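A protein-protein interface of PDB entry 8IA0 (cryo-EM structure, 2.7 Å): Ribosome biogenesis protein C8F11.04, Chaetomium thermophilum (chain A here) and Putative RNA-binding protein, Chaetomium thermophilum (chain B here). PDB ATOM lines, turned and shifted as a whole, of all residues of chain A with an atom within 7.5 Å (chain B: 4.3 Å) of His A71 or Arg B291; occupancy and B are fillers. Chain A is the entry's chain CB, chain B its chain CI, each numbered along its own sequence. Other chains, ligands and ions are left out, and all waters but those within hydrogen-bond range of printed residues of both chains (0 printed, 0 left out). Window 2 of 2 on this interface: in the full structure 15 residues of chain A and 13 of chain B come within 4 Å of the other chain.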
ATOM      1  N   THR A  68     -12.530 -23.168 -11.105  1.00  0.00           N
ATOM      2  CA  THR A  68     -11.480 -22.443 -11.807  1.00  0.00           C
ATOM      3  C   THR A  68     -11.829 -22.280 -13.282  1.00  0.00           C
ATOM      4  O   THR A  68     -12.898 -22.682 -13.751  1.00  0.00           O
ATOM      5  CB  THR A  68     -10.120 -23.132 -11.675  1.00  0.00           C
ATOM      6  OG1 THR A  68     -10.011 -24.178 -12.649  1.00  0.00           O
ATOM      7  CG2 THR A  68      -9.917 -23.681 -10.310  1.00  0.00           C
ATOM      8  N   LYS A  69     -10.893 -21.674 -14.012  1.00  0.00           N
ATOM      9  CA  LYS A  69     -10.982 -21.499 -15.454  1.00  0.00           C
ATOM     10  C   LYS A  69      -9.947 -22.347 -16.185  1.00  0.00           C
ATOM     11  O   LYS A  69      -9.680 -22.112 -17.367  1.00  0.00           O
ATOM     12  CB  LYS A  69     -10.831 -20.019 -15.810  1.00  0.00           C
ATOM     13  CG  LYS A  69      -9.598 -19.373 -15.211  1.00  0.00           C
ATOM     14  CD  LYS A  69      -9.425 -17.947 -15.694  1.00  0.00           C
ATOM     15  CE  LYS A  69     -10.463 -17.038 -15.057  1.00  0.00           C
ATOM     16  NZ  LYS A  69     -10.235 -16.898 -13.589  1.00  0.00           N
ATOM     17  N   LYS A  70      -9.355 -23.322 -15.499  1.00  0.00           N
ATOM     18  CA  LYS A  70      -8.432 -24.255 -16.129  1.00  0.00           C
ATOM     19  C   LYS A  70      -8.285 -25.482 -15.239  1.00  0.00           C
ATOM     20  O   LYS A  70      -8.648 -25.465 -14.060  1.00  0.00           O
ATOM     21  CB  LYS A  70      -7.072 -23.601 -16.407  1.00  0.00           C
ATOM     22  CG  LYS A  70      -6.236 -24.278 -17.500  1.00  0.00           C
ATOM     23  CD  LYS A  70      -7.096 -24.956 -18.571  1.00  0.00           C
ATOM     24  CE  LYS A  70      -7.898 -23.964 -19.410  1.00  0.00           C
ATOM     25  NZ  LYS A  70      -8.815 -24.681 -20.337  1.00  0.00           N
ATOM     26  N   HIS A  71      -7.754 -26.549 -15.830  1.00  0.00           N
ATOM     27  CA  HIS A  71      -7.601 -27.813 -15.125  1.00  0.00           C
ATOM     28  C   HIS A  71      -6.657 -27.677 -13.939  1.00  0.00           C
ATOM     29  O   HIS A  71      -5.635 -26.988 -14.010  1.00  0.00           O
ATOM     30  CB  HIS A  71      -7.072 -28.881 -16.079  1.00  0.00           C
ATOM     31  CG  HIS A  71      -7.875 -29.027 -17.332  1.00  0.00           C
ATOM     32  ND1 HIS A  71      -7.364 -28.742 -18.579  1.00  0.00           N
ATOM     33  CD2 HIS A  71      -9.155 -29.421 -17.530  1.00  0.00           C
ATOM     34  CE1 HIS A  71      -8.291 -28.961 -19.493  1.00  0.00           C
ATOM     35  NE2 HIS A  71      -9.388 -29.375 -18.882  1.00  0.00           N
ATOM     36  N   ILE A  72      -7.010 -28.342 -12.838  1.00  0.00           N
ATOM     37  CA  ILE A  72      -6.095 -28.442 -11.704  1.00  0.00           C
ATOM     38  C   ILE A  72      -4.909 -29.326 -12.059  1.00  0.00           C
ATOM     39  O   ILE A  72      -3.770 -29.051 -11.663  1.00  0.00           O
ATOM     40  CB  ILE A  72      -6.826 -28.964 -10.450  1.00  0.00           C
ATOM     41  CG1 ILE A  72      -8.116 -28.184 -10.152  1.00  0.00           C
ATOM     42  CG2 ILE A  72      -5.905 -28.930  -9.240  1.00  0.00           C
ATOM     43  CD1 ILE A  72      -8.111 -26.721 -10.558  1.00  0.00           C
ATOM     44  N   HIS A  73      -5.153 -30.394 -12.814  1.00  0.00           N
ATOM     45  CA  HIS A  73      -4.120 -31.356 -13.164  1.00  0.00           C
ATOM     46  C   HIS A  73      -4.344 -31.816 -14.595  1.00  0.00           C
ATOM     47  O   HIS A  73      -5.438 -31.682 -15.147  1.00  0.00           O
ATOM     48  CB  HIS A  73      -4.130 -32.556 -12.209  1.00  0.00           C
ATOM     49  CG  HIS A  73      -2.776 -33.131 -11.939  1.00  0.00           C
ATOM     50  ND1 HIS A  73      -2.161 -34.022 -12.791  1.00  0.00           N
ATOM     51  CD2 HIS A  73      -1.926 -32.957 -10.901  1.00  0.00           C
ATOM     52  CE1 HIS A  73      -0.987 -34.365 -12.295  1.00  0.00           C
ATOM     53  NE2 HIS A  73      -0.819 -33.732 -11.148  1.00  0.00           N
ATOM     54  N   ASP A  74      -3.286 -32.359 -15.198  1.00  0.00           N
ATOM     55  CA  ASP A  74      -3.401 -32.864 -16.562  1.00  0.00           C
ATOM     56  C   ASP A  74      -4.268 -34.116 -16.620  1.00  0.00           C
ATOM     57  O   ASP A  74      -5.070 -34.278 -17.547  1.00  0.00           O
ATOM     58  CB  ASP A  74      -2.012 -33.141 -17.140  1.00  0.00           C
ATOM     59  CG  ASP A  74      -1.146 -33.970 -16.212  1.00  0.00           C
ATOM     60  OD1 ASP A  74      -1.673 -34.486 -15.205  1.00  0.00           O
ATOM     61  OD2 ASP A  74       0.063 -34.105 -16.490  1.00  0.00           O
ATOM     62  N   SER A  75      -4.124 -35.009 -15.644  1.00  0.00           N
ATOM     63  CA  SER A  75      -4.892 -36.243 -15.579  1.00  0.00           C
ATOM     64  C   SER A  75      -5.341 -36.483 -14.141  1.00  0.00           C
ATOM     65  O   SER A  75      -5.042 -35.701 -13.234  1.00  0.00           O
ATOM     66  CB  SER A  75      -4.077 -37.433 -16.099  1.00  0.00           C
ATOM     67  OG  SER A  75      -3.095 -37.822 -15.157  1.00  0.00           O
ATOM     68  N   SER A 236      -8.508 -33.758  -9.551  1.00  0.00           N
ATOM     69  CA  SER A 236      -9.205 -34.241 -10.728  1.00  0.00           C
ATOM     70  C   SER A 236      -8.880 -33.356 -11.929  1.00  0.00           C
ATOM     71  O   SER A 236      -8.556 -32.176 -11.773  1.00  0.00           O
ATOM     72  CB  SER A 236     -10.712 -34.260 -10.486  1.00  0.00           C
ATOM     73  OG  SER A 236     -11.217 -32.949 -10.299  1.00  0.00           O
ATOM     74  N   PRO A 237      -8.944 -33.909 -13.142  1.00  0.00           N
ATOM     75  CA  PRO A 237      -8.661 -33.091 -14.330  1.00  0.00           C
ATOM     76  C   PRO A 237      -9.587 -31.901 -14.492  1.00  0.00           C
ATOM     77  O   PRO A 237      -9.169 -30.888 -15.060  1.00  0.00           O
ATOM     78  CB  PRO A 237      -8.826 -34.088 -15.483  1.00  0.00           C
ATOM     79  CG  PRO A 237      -8.526 -35.402 -14.875  1.00  0.00           C
ATOM     80  CD  PRO A 237      -9.082 -35.334 -13.480  1.00  0.00           C
ATOM     81  N   SER A 238     -10.821 -31.978 -14.005  1.00  0.00           N
ATOM     82  CA  SER A 238     -11.804 -30.946 -14.299  1.00  0.00           C
ATOM     83  C   SER A 238     -11.471 -29.646 -13.572  1.00  0.00           C
ATOM     84  O   SER A 238     -10.468 -29.525 -12.864  1.00  0.00           O
ATOM     85  CB  SER A 238     -13.202 -31.417 -13.916  1.00  0.00           C
ATOM     86  OG  SER A 238     -13.593 -30.882 -12.664  1.00  0.00           O
ATOM     87  N   THR A 239     -12.348 -28.659 -13.757  1.00  0.00           N
ATOM     88  CA  THR A 239     -12.208 -27.340 -13.158  1.00  0.00           C
ATOM     89  C   THR A 239     -13.084 -27.173 -11.922  1.00  0.00           C
ATOM     90  O   THR A 239     -13.400 -26.045 -11.530  1.00  0.00           O
ATOM     91  CB  THR A 239     -12.533 -26.258 -14.187  1.00  0.00           C
ATOM     92  OG1 THR A 239     -13.926 -26.320 -14.521  1.00  0.00           O
ATOM     93  CG2 THR A 239     -11.710 -26.461 -15.449  1.00  0.00           C
ATOM     94  N   ASN A 240     -13.484 -28.279 -11.300  1.00  0.00           N
ATOM     95  CA  ASN A 240     -14.324 -28.248 -10.108  1.00  0.00           C
ATOM     96  C   ASN A 240     -13.777 -29.250  -9.106  1.00  0.00           C
ATOM     97  O   ASN A 240     -13.692 -30.445  -9.408  1.00  0.00           O
ATOM     98  CB  ASN A 240     -15.781 -28.569 -10.448  1.00  0.00           C
ATOM     99  CG  ASN A 240     -16.700 -28.465  -9.246  1.00  0.00           C
ATOM    100  OD1 ASN A 240     -16.285 -28.055  -8.162  1.00  0.00           O
ATOM    101  ND2 ASN A 240     -17.957 -28.850  -9.430  1.00  0.00           N
ATOM    102  N   PHE A 270      -1.975 -26.090  -4.647  1.00  0.00           N
ATOM    103  CA  PHE A 270      -2.436 -27.084  -5.608  1.00  0.00           C
ATOM    104  C   PHE A 270      -2.833 -26.502  -6.956  1.00  0.00           C
ATOM    105  O   PHE A 270      -2.331 -26.956  -7.989  1.00  0.00           O
ATOM    106  CB  PHE A 270      -3.608 -27.873  -5.010  1.00  0.00           C
ATOM    107  CG  PHE A 270      -3.191 -28.856  -3.958  1.00  0.00           C
ATOM    108  CD1 PHE A 270      -2.638 -30.073  -4.314  1.00  0.00           C
ATOM    109  CD2 PHE A 270      -3.332 -28.558  -2.615  1.00  0.00           C
ATOM    110  CE1 PHE A 270      -2.245 -30.979  -3.350  1.00  0.00           C
ATOM    111  CE2 PHE A 270      -2.939 -29.459  -1.647  1.00  0.00           C
ATOM    112  CZ  PHE A 270      -2.395 -30.671  -2.015  1.00  0.00           C
ATOM    113  N   VAL A 271      -3.724 -25.516  -6.988  1.00  0.00           N
ATOM    114  CA  VAL A 271      -4.205 -24.986  -8.262  1.00  0.00           C
ATOM    115  C   VAL A 271      -3.092 -24.186  -8.927  1.00  0.00           C
ATOM    116  O   VAL A 271      -2.522 -23.277  -8.307  1.00  0.00           O
ATOM    117  CB  VAL A 271      -5.475 -24.140  -8.080  1.00  0.00           C
ATOM    118  CG1 VAL A 271      -5.313 -23.168  -6.935  1.00  0.00           C
ATOM    119  CG2 VAL A 271      -5.808 -23.400  -9.367  1.00  0.00           C
ATOM    120  N   PRO A 272      -2.735 -24.500 -10.169  1.00  0.00           N
ATOM    121  CA  PRO A 272      -1.705 -23.719 -10.859  1.00  0.00           C
ATOM    122  C   PRO A 272      -2.183 -22.304 -11.140  1.00  0.00           C
ATOM    123  O   PRO A 272      -3.383 -22.038 -11.236  1.00  0.00           O
ATOM    124  CB  PRO A 272      -1.476 -24.500 -12.157  1.00  0.00           C
ATOM    125  CG  PRO A 272      -2.754 -25.235 -12.379  1.00  0.00           C
ATOM    126  CD  PRO A 272      -3.266 -25.585 -11.011  1.00  0.00           C
ATOM    127  N   GLN A 273      -1.218 -21.390 -11.253  1.00  0.00           N
ATOM    128  CA  GLN A 273      -1.405 -19.961 -11.489  1.00  0.00           C
ATOM    129  C   GLN A 273      -2.057 -19.244 -10.312  1.00  0.00           C
ATOM    130  O   GLN A 273      -2.332 -18.042 -10.417  1.00  0.00           O
ATOM    131  CB  GLN A 273      -2.213 -19.676 -12.765  1.00  0.00           C
ATOM    132  CG  GLN A 273      -1.417 -19.859 -14.047  1.00  0.00           C
ATOM    133  CD  GLN A 273      -1.383 -21.299 -14.515  1.00  0.00           C
ATOM    134  OE1 GLN A 273      -2.292 -22.079 -14.230  1.00  0.00           O
ATOM    135  NE2 GLN A 273      -0.328 -21.661 -15.235  1.00  0.00           N
ATOM    136  N   ASN A 277      -5.976 -18.139 -11.625  1.00  0.00           N
ATOM    137  CA  ASN A 277      -6.788 -19.246 -12.108  1.00  0.00           C
ATOM    138  C   ASN A 277      -8.027 -19.492 -11.259  1.00  0.00           C
ATOM    139  O   ASN A 277      -8.924 -20.213 -11.705  1.00  0.00           O
ATOM    140  CB  ASN A 277      -5.937 -20.517 -12.161  1.00  0.00           C
ATOM    141  CG  ASN A 277      -6.447 -21.524 -13.172  1.00  0.00           C
ATOM    142  OD1 ASN A 277      -7.422 -21.276 -13.878  1.00  0.00           O
ATOM    143  ND2 ASN A 277      -5.779 -22.670 -13.251  1.00  0.00           N
ATOM    144  N   LYS B 287      -9.882 -34.179 -22.618  1.00  0.00           N
ATOM    145  CA  LYS B 287      -8.779 -33.355 -23.095  1.00  0.00           C
ATOM    146  C   LYS B 287      -9.246 -32.375 -24.163  1.00  0.00           C
ATOM    147  O   LYS B 287      -8.859 -31.201 -24.150  1.00  0.00           O
ATOM    148  CB  LYS B 287      -7.658 -34.243 -23.632  1.00  0.00           C
ATOM    149  CG  LYS B 287      -7.050 -35.169 -22.588  1.00  0.00           C
ATOM    150  CD  LYS B 287      -5.556 -35.396 -22.804  1.00  0.00           C
ATOM    151  CE  LYS B 287      -4.797 -34.118 -23.156  1.00  0.00           C
ATOM    152  NZ  LYS B 287      -5.148 -32.955 -22.289  1.00  0.00           N
ATOM    153  N   MET B 288     -10.074 -32.837 -25.101  1.00  0.00           N
ATOM    154  CA  MET B 288     -10.531 -31.966 -26.180  1.00  0.00           C
ATOM    155  C   MET B 288     -11.431 -30.856 -25.651  1.00  0.00           C
ATOM    156  O   MET B 288     -11.214 -29.673 -25.941  1.00  0.00           O
ATOM    157  CB  MET B 288     -11.262 -32.783 -27.245  1.00  0.00           C
ATOM    158  CG  MET B 288     -10.423 -33.867 -27.894  1.00  0.00           C
ATOM    159  SD  MET B 288     -11.029 -34.308 -29.535  1.00  0.00           S
ATOM    160  CE  MET B 288     -11.467 -32.695 -30.181  1.00  0.00           C
ATOM    161  N   ALA B 289     -12.451 -31.219 -24.872  1.00  0.00           N
ATOM    162  CA  ALA B 289     -13.355 -30.212 -24.330  1.00  0.00           C
ATOM    163  C   ALA B 289     -12.638 -29.301 -23.346  1.00  0.00           C
ATOM    164  O   ALA B 289     -12.869 -28.086 -23.327  1.00  0.00           O
ATOM    165  CB  ALA B 289     -14.556 -30.884 -23.664  1.00  0.00           C
ATOM    166  N   GLY B 290     -11.765 -29.872 -22.515  1.00  0.00           N
ATOM    167  CA  GLY B 290     -11.087 -29.075 -21.509  1.00  0.00           C
ATOM    168  C   GLY B 290     -10.126 -28.059 -22.095  1.00  0.00           C
ATOM    169  O   GLY B 290     -10.089 -26.906 -21.658  1.00  0.00           O
ATOM    170  N   ARG B 291      -9.329 -28.469 -23.085  1.00  0.00           N
ATOM    171  CA  ARG B 291      -8.389 -27.535 -23.693  1.00  0.00           C
ATOM    172  C   ARG B 291      -9.086 -26.528 -24.592  1.00  0.00           C
ATOM    173  O   ARG B 291      -8.568 -25.425 -24.798  1.00  0.00           O
ATOM    174  CB  ARG B 291      -7.334 -28.274 -24.507  1.00  0.00           C
ATOM    175  CG  ARG B 291      -6.029 -27.513 -24.606  1.00  0.00           C
ATOM    176  CD  ARG B 291      -4.916 -28.439 -25.003  1.00  0.00           C
ATOM    177  NE  ARG B 291      -4.925 -28.605 -26.448  1.00  0.00           N
ATOM    178  CZ  ARG B 291      -4.536 -29.701 -27.083  1.00  0.00           C
ATOM    179  NH1 ARG B 291      -4.112 -30.767 -26.426  1.00  0.00           N
ATOM    180  NH2 ARG B 291      -4.584 -29.728 -28.410  1.00  0.00           N
ATOM    181  N   GLN B 292     -10.246 -26.887 -25.145  1.00  0.00           N
ATOM    182  CA  GLN B 292     -11.039 -25.909 -25.879  1.00  0.00           C
ATOM    183  C   GLN B 292     -11.414 -24.735 -24.987  1.00  0.00           C
ATOM    184  O   GLN B 292     -11.668 -23.632 -25.482  1.00  0.00           O
ATOM    185  CB  GLN B 292     -12.291 -26.578 -26.447  1.00  0.00           C
ATOM    186  CG  GLN B 292     -13.068 -25.725 -27.430  1.00  0.00           C
ATOM    187  CD  GLN B 292     -14.162 -24.924 -26.757  1.00  0.00           C
ATOM    188  OE1 GLN B 292     -14.730 -25.352 -25.751  1.00  0.00           O
ATOM    189  NE2 GLN B 292     -14.463 -23.753 -27.303  1.00  0.00           N
ATOM    190  N   LEU B 293     -11.438 -24.955 -23.673  1.00  0.00           N
ATOM    191  CA  LEU B 293     -11.669 -23.861 -22.740  1.00  0.00           C
ATOM    192  C   LEU B 293     -10.420 -23.000 -22.590  1.00  0.00           C
ATOM    193  O   LEU B 293     -10.491 -21.878 -22.076  1.00  0.00           O
ATOM    194  CB  LEU B 293     -12.116 -24.431 -21.392  1.00  0.00           C
ATOM    195  CG  LEU B 293     -12.865 -23.538 -20.404  1.00  0.00           C
ATOM    196  CD1 LEU B 293     -13.934 -24.349 -19.690  1.00  0.00           C
ATOM    197  CD2 LEU B 293     -11.911 -22.929 -19.401  1.00  0.00           C
ATOM    198  N   GLU B 294      -9.269 -23.502 -23.043  1.00  0.00           N
ATOM    199  CA  GLU B 294      -8.010 -22.772 -22.957  1.00  0.00           C
ATOM    200  C   GLU B 294      -7.759 -21.899 -24.180  1.00  0.00           C
ATOM    201  O   GLU B 294      -7.229 -20.793 -24.029  1.00  0.00           O
ATOM    202  CB  GLU B 294      -6.855 -23.775 -22.737  1.00  0.00           C
ATOM    203  CG  GLU B 294      -5.389 -23.267 -22.591  1.00  0.00           C
ATOM    204  CD  GLU B 294      -4.853 -22.409 -23.727  1.00  0.00           C
ATOM    205  OE1 GLU B 294      -5.149 -22.708 -24.903  1.00  0.00           O
ATOM    206  OE2 GLU B 294      -4.134 -21.429 -23.438  1.00  0.00           O
ATOM    207  N   ARG B 295      -8.137 -22.357 -25.372  1.00  0.00           N
ATOM    208  CA  ARG B 295      -7.783 -21.642 -26.590  1.00  0.00           C
ATOM    209  C   ARG B 295      -8.407 -20.248 -26.597  1.00  0.00           C
ATOM    210  O   ARG B 295      -9.611 -20.098 -26.365  1.00  0.00           O
ATOM    211  CB  ARG B 295      -8.224 -22.434 -27.825  1.00  0.00           C
ATOM    212  CG  ARG B 295      -9.714 -22.732 -27.904  1.00  0.00           C
ATOM    213  CD  ARG B 295     -10.051 -23.575 -29.124  1.00  0.00           C
ATOM    214  NE  ARG B 295      -9.871 -22.837 -30.368  1.00  0.00           N
ATOM    215  CZ  ARG B 295      -9.891 -23.388 -31.573  1.00  0.00           C
ATOM    216  NH1 ARG B 295     -10.080 -24.687 -31.737  1.00  0.00           N
ATOM    217  NH2 ARG B 295      -9.718 -22.615 -32.642  1.00  0.00           N
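Hydrophobic or aromatic side chains of chain A that line the printed part of chain B: His A71.
Of the 9 printed residues of chain B, 4 touch a printed residue of chain A.
Hydrophobic or aromatic side chains of chain B that line the printed part of chain A: Leu B293.
Among the printed residues, pairs that only touch across the chains: Lys A69 with Leu B293 (3.1 Å), His A71 with Gly B290 (3.1 Å), Lys A70 with Leu B293 (3.2 Å) and His A71 with Arg B291 (3.8 Å).
Of chain B, only Gly B290 (3.1 Å) and Arg B291 (3.8 Å) come within 4 Å of His A71.
Of chain A, only His A71 (3.8 Å) comes within 4 Å of Arg B291.
Of chain A, only Lys A70 (2.9 Å) and His A71 (3.1 Å) come within 4 Å of Gly B290.
Of the printed residues of chain B, Lys A70 touches Gly B290, Leu B293 and Glu B294.
Of the printed residues of chain B, Lys A69 touches Leu B293.
Of the printed residues of chain A, Glu B294 touches Lys A70.
Of the printed residues of chain A, Leu B293 touches Lys A69 and Lys A70.
Gln B292 touches none of the printed residues of chain A.
Ala B289 touches none of the printed residues of chain A.
The nearest residue of chain A that does not touch Arg B291 is Lys A70 (4.4 Å).
The backbone carbonyl oxygen (O) of Gly B290 lies within hydrogen-bond range of the side-chain amino group (NZ) of Lys A70, at 2.9 Å.
The side-chain amino group of Lys A70 sits close to the backbone NH of Glu B294 (3.0 Å).
N of Lys A70 is in hydrogen-bond range of OG1 of Thr A68 (3.0 Å).
N of Lys A69 is in hydrogen-bond range of O of Asn A277, 3.4 Å away.
OD1 of Asn A277 lies within hydrogen-bond range of N of Lys A70 (3.2 Å).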
